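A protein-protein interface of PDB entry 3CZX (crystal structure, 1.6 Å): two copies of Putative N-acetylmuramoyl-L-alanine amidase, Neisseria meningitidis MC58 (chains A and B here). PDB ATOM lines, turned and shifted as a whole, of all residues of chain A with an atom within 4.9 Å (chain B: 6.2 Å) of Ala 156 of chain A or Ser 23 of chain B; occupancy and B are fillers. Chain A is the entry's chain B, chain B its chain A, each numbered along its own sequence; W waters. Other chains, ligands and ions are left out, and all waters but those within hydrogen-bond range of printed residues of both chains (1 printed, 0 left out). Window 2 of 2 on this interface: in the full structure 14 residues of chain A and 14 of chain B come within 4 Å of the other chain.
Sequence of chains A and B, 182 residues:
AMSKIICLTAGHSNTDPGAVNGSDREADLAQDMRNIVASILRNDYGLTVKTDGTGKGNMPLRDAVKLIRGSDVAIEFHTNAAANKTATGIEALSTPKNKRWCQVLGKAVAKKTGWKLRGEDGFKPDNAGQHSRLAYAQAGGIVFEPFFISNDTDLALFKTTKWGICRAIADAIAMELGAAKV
The side-chain hydroxyl (OG) of Ser 23 of chain B sits at hydrogen-bond distance from the side-chain amino group (NZ) of Lys 159 of chain A, 3.0 Å away.
The side-chain carboxylate of Asp 24 of chain B is in salt-bridge range of the side-chain amino group of Lys 159 of chain A (2.7 Å).
NH2 of Arg 25 of chain B is in salt-bridge range of OD1 of Asp 28 of chain B.
The side-chain carboxylate of Asp 24 of chain A lies within salt-bridge range of the side-chain amino group of Lys 159 of chain A.
OG1 of Thr 160 of chain A is in hydrogen-bond range of O of Ala 156 of chain A, at 3.3 Å.
O of Leu 157 of chain A is in hydrogen-bond range of OG1 of Thr 160 of chain A (3.4 Å).
Among the printed residues, pairs that only touch across the chains: Thr 160 of chain A with Asp 28 of chain B (3.4 Å), Thr 160 of chain A with Arg 25 of chain B (3.6 Å), Ala 156 of chain A with Ser 23 of chain B (3.7 Å) and Lys 159 of chain A with Asp 28 of chain B (3.8 Å).
Asn 151 of chain A touches none of the printed residues of chain B.
Printed residues of chain B within 4 Å of Lys 159 of chain A: Ser 23 (3.0 Å), Asp 24 (2.7 Å) and Asp 28 (3.8 Å).
Ser 23 of chain B touches two residues of chain A.
Of the printed residues of chain A, Arg 25 of chain B touches Thr 160.
Of the printed residues of chain A, Asp 28 of chain B touches Lys 159 and Thr 160.
The nearest residue of chain A that does not touch Ser 23 of chain B is Asp 24 of chain A (4.7 Å).
The nearest printed residue of chain B that does not touch Lys 159 of chain A is Asn 21 of chain B (5.8 Å).
Of the 6 printed residues of chain B, 4 touch a printed residue of chain A.
Printed residues of chain B that touch a printed residue of chain A: Ser 23, Asp 24, Arg 25 and Asp 28.
Along chain A the printed residues that touch a printed residue of chain B span positions 156 to 160.
Position printed for both chains: 24.
Water W1 lies within hydrogen-bond range of O of Asp 152 of chain A (2.8 Å) and OG of Ser 23 of chain B (2.9 Å).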
ATOM      1  N   ASP A  24      25.427  -9.970   7.445  1.00  0.00           N
ATOM      2  CA  ASP A  24      26.376  -9.137   6.704  1.00  0.00           C
ATOM      3  C   ASP A  24      27.744  -9.815   6.730  1.00  0.00           C
ATOM      4  O   ASP A  24      28.225 -10.203   7.782  1.00  0.00           O
ATOM      5  CB  ASP A  24      26.420  -7.738   7.283  1.00  0.00           C
ATOM      6  CG  ASP A  24      25.133  -6.972   7.026  1.00  0.00           C
ATOM      7  OD1 ASP A  24      24.877  -6.666   5.852  1.00  0.00           O
ATOM      8  OD2 ASP A  24      24.439  -6.620   8.007  1.00  0.00           O
ATOM      9  N   ASN A 151      31.288  -3.424  14.231  1.00  0.00           N
ATOM     10  CA  ASN A 151      30.674  -2.258  14.862  1.00  0.00           C
ATOM     11  C   ASN A 151      29.301  -2.027  14.284  1.00  0.00           C
ATOM     12  O   ASN A 151      29.180  -1.578  13.138  1.00  0.00           O
ATOM     13  CB  ASN A 151      31.568  -1.028  14.704  1.00  0.00           C
ATOM     14  CG  ASN A 151      31.055   0.167  15.498  1.00  0.00           C
ATOM     15  OD1 ASN A 151      29.922   0.598  15.294  1.00  0.00           O
ATOM     16  ND2 ASN A 151      31.911   0.730  16.390  1.00  0.00           N
ATOM     17  N   ASP A 152      28.249  -2.372  15.025  1.00  0.00           N
ATOM     18  CA  ASP A 152      26.898  -2.282  14.428  1.00  0.00           C
ATOM     19  C   ASP A 152      26.561  -0.900  13.860  1.00  0.00           C
ATOM     20  O   ASP A 152      25.917  -0.782  12.793  1.00  0.00           O
ATOM     21  CB  ASP A 152      25.792  -2.676  15.427  1.00  0.00           C
ATOM     22  CG  ASP A 152      25.778  -4.143  15.778  1.00  0.00           C
ATOM     23  OD1 ASP A 152      26.411  -4.998  15.119  1.00  0.00           O
ATOM     24  OD2 ASP A 152      25.093  -4.482  16.781  1.00  0.00           O
ATOM     25  N   THR A 153      26.955   0.150  14.582  1.00  0.00           N
ATOM     26  CA  THR A 153      26.626   1.508  14.230  1.00  0.00           C
ATOM     27  C   THR A 153      27.334   1.901  12.947  1.00  0.00           C
ATOM     28  O   THR A 153      26.677   2.427  12.042  1.00  0.00           O
ATOM     29  CB  THR A 153      27.013   2.526  15.340  1.00  0.00           C
ATOM     30  OG1 THR A 153      26.305   2.182  16.540  1.00  0.00           O
ATOM     31  CG2 THR A 153      26.656   3.931  14.938  1.00  0.00           C
ATOM     32  N   ASP A 154      28.620   1.560  12.841  1.00  0.00           N
ATOM     33  CA  ASP A 154      29.408   1.969  11.628  1.00  0.00           C
ATOM     34  C   ASP A 154      28.957   1.122  10.419  1.00  0.00           C
ATOM     35  O   ASP A 154      28.813   1.650   9.300  1.00  0.00           O
ATOM     36  CB  ASP A 154      30.927   1.858  11.821  1.00  0.00           C
ATOM     37  CG  ASP A 154      31.442   2.655  13.042  1.00  0.00           C
ATOM     38  OD1 ASP A 154      30.768   3.601  13.477  1.00  0.00           O
ATOM     39  OD2 ASP A 154      32.508   2.270  13.543  1.00  0.00           O
ATOM     40  N   LEU A 155      28.679  -0.142  10.654  1.00  0.00           N
ATOM     41  CA  LEU A 155      28.148  -1.024   9.578  1.00  0.00           C
ATOM     42  C   LEU A 155      26.831  -0.490   9.081  1.00  0.00           C
ATOM     43  O   LEU A 155      26.575  -0.418   7.856  1.00  0.00           O
ATOM     44  CB  LEU A 155      28.033  -2.460  10.072  1.00  0.00           C
ATOM     45  CG  LEU A 155      27.247  -3.437   9.193  1.00  0.00           C
ATOM     46  CD1 LEU A 155      27.953  -3.587   7.847  1.00  0.00           C
ATOM     47  CD2 LEU A 155      27.089  -4.801   9.896  1.00  0.00           C
ATOM     48  N   ALA A 156      25.953  -0.076  10.004  1.00  0.00           N
ATOM     49  CA  ALA A 156      24.674   0.516   9.559  1.00  0.00           C
ATOM     50  C   ALA A 156      24.880   1.767   8.708  1.00  0.00           C
ATOM     51  O   ALA A 156      24.182   1.976   7.697  1.00  0.00           O
ATOM     52  CB  ALA A 156      23.730   0.829  10.744  1.00  0.00           C
ATOM     53  N   LEU A 157      25.826   2.617   9.094  1.00  0.00           N
ATOM     54  CA  LEU A 157      26.112   3.829   8.326  1.00  0.00           C
ATOM     55  C   LEU A 157      26.601   3.452   6.944  1.00  0.00           C
ATOM     56  O   LEU A 157      26.204   4.058   5.944  1.00  0.00           O
ATOM     57  CB  LEU A 157      27.105   4.753   9.052  1.00  0.00           C
ATOM     58  CG  LEU A 157      27.311   6.093   8.363  1.00  0.00           C
ATOM     59  CD1 LEU A 157      25.953   6.868   8.329  1.00  0.00           C
ATOM     60  CD2 LEU A 157      28.405   6.912   9.087  1.00  0.00           C
ATOM     61  N   PHE A 158      27.468   2.456   6.879  1.00  0.00           N
ATOM     62  CA  PHE A 158      27.944   2.044   5.556  1.00  0.00           C
ATOM     63  C   PHE A 158      26.759   1.618   4.722  1.00  0.00           C
ATOM     64  O   PHE A 158      26.667   1.968   3.551  1.00  0.00           O
ATOM     65  CB  PHE A 158      28.933   0.920   5.648  1.00  0.00           C
ATOM     66  CG  PHE A 158      29.345   0.395   4.304  1.00  0.00           C
ATOM     67  CD1 PHE A 158      30.256   1.083   3.529  1.00  0.00           C
ATOM     68  CD2 PHE A 158      28.789  -0.756   3.810  1.00  0.00           C
ATOM     69  CE1 PHE A 158      30.624   0.578   2.244  1.00  0.00           C
ATOM     70  CE2 PHE A 158      29.124  -1.230   2.534  1.00  0.00           C
ATOM     71  CZ  PHE A 158      30.055  -0.573   1.781  1.00  0.00           C
ATOM     72  N   LYS A 159      25.909   0.781   5.307  1.00  0.00           N
ATOM     73  CA  LYS A 159      24.777   0.210   4.564  1.00  0.00           C
ATOM     74  C   LYS A 159      23.855   1.292   4.020  1.00  0.00           C
ATOM     75  O   LYS A 159      23.360   1.188   2.885  1.00  0.00           O
ATOM     76  CB  LYS A 159      24.022  -0.801   5.422  1.00  0.00           C
ATOM     77  CG  LYS A 159      24.825  -2.055   5.668  1.00  0.00           C
ATOM     78  CD  LYS A 159      24.262  -2.939   6.767  1.00  0.00           C
ATOM     79  CE  LYS A 159      23.034  -3.649   6.405  1.00  0.00           C
ATOM     80  NZ  LYS A 159      22.680  -4.678   7.473  1.00  0.00           N
ATOM     81  N   THR A 160      23.633   2.364   4.796  1.00  0.00           N
ATOM     82  CA  THR A 160      22.698   3.414   4.377  1.00  0.00           C
ATOM     83  C   THR A 160      23.316   4.495   3.511  1.00  0.00           C
ATOM     84  O   THR A 160      22.586   5.227   2.827  1.00  0.00           O
ATOM     85  CB  THR A 160      21.966   4.066   5.592  1.00  0.00           C
ATOM     86  OG1 THR A 160      22.907   4.743   6.447  1.00  0.00           O
ATOM     87  CG2 THR A 160      21.243   2.998   6.394  1.00  0.00           C
ATOM     88  N   ASN B  21      14.456  -4.346   8.504  1.00  0.00           N
ATOM     89  CA  ASN B  21      14.759  -5.525   9.266  1.00  0.00           C
ATOM     90  C   ASN B  21      16.161  -5.291   9.819  1.00  0.00           C
ATOM     91  O   ASN B  21      17.151  -5.408   9.111  1.00  0.00           O
ATOM     92  CB  ASN B  21      14.657  -6.791   8.389  1.00  0.00           C
ATOM     93  CG  ASN B  21      14.884  -8.088   9.163  1.00  0.00           C
ATOM     94  OD1 ASN B  21      15.441  -8.090  10.275  1.00  0.00           O
ATOM     95  ND2 ASN B  21      14.486  -9.206   8.574  1.00  0.00           N
ATOM     96  N   GLY B  22      16.255  -4.934  11.092  1.00  0.00           N
ATOM     97  CA  GLY B  22      17.553  -4.534  11.633  1.00  0.00           C
ATOM     98  C   GLY B  22      18.035  -3.287  10.933  1.00  0.00           C
ATOM     99  O   GLY B  22      17.267  -2.313  10.770  1.00  0.00           O
ATOM    100  N   SER B  23      19.298  -3.299  10.498  1.00  0.00           N
ATOM    101  CA  SER B  23      19.832  -2.166   9.743  1.00  0.00           C
ATOM    102  C   SER B  23      19.667  -2.343   8.233  1.00  0.00           C
ATOM    103  O   SER B  23      20.168  -1.516   7.475  1.00  0.00           O
ATOM    104  CB  SER B  23      21.291  -1.868  10.105  1.00  0.00           C
ATOM    105  OG  SER B  23      22.107  -2.985   9.863  1.00  0.00           O
ATOM    106  N   ASP B  24      18.969  -3.401   7.820  1.00  0.00           N
ATOM    107  CA  ASP B  24      18.571  -3.534   6.424  1.00  0.00           C
ATOM    108  C   ASP B  24      17.282  -2.767   6.158  1.00  0.00           C
ATOM    109  O   ASP B  24      16.256  -2.999   6.810  1.00  0.00           O
ATOM    110  CB  ASP B  24      18.397  -5.006   6.079  1.00  0.00           C
ATOM    111  CG  ASP B  24      19.719  -5.764   6.163  1.00  0.00           C
ATOM    112  OD1 ASP B  24      20.727  -5.260   5.660  1.00  0.00           O
ATOM    113  OD2 ASP B  24      19.735  -6.856   6.730  1.00  0.00           O
ATOM    114  N   ARG B  25      17.331  -1.873   5.176  1.00  0.00           N
ATOM    115  CA  ARG B  25      16.192  -1.031   4.828  1.00  0.00           C
ATOM    116  C   ARG B  25      15.753  -1.280   3.393  1.00  0.00           C
ATOM    117  O   ARG B  25      16.586  -1.285   2.484  1.00  0.00           O
ATOM    118  CB  ARG B  25      16.546   0.435   4.932  1.00  0.00           C
ATOM    119  CG  ARG B  25      17.117   0.880   6.311  1.00  0.00           C
ATOM    120  CD  ARG B  25      17.100   2.402   6.411  1.00  0.00           C
ATOM    121  NE  ARG B  25      17.840   3.037   5.326  1.00  0.00           N
ATOM    122  CZ  ARG B  25      17.823   4.340   5.053  1.00  0.00           C
ATOM    123  NH1 ARG B  25      17.098   5.214   5.774  1.00  0.00           N
ATOM    124  NH2 ARG B  25      18.508   4.782   4.020  1.00  0.00           N
ATOM    125  N   ASP B  28      17.209   0.875   0.689  1.00  0.00           N
ATOM    126  CA  ASP B  28      18.613   0.632   0.357  1.00  0.00           C
ATOM    127  C   ASP B  28      18.675  -0.573  -0.544  1.00  0.00           C
ATOM    128  O   ASP B  28      19.486  -0.600  -1.482  1.00  0.00           O
ATOM    129  CB  ASP B  28      19.421   0.396   1.646  1.00  0.00           C
ATOM    130  CG  ASP B  28      19.422   1.622   2.569  1.00  0.00           C
ATOM    131  OD1 ASP B  28      19.184   2.757   2.091  1.00  0.00           O
ATOM    132  OD2 ASP B  28      19.676   1.428   3.780  1.00  0.00           O
HETATM  133  O   HOH W   1      24.163  -2.699  11.866  1.00  0.00           O
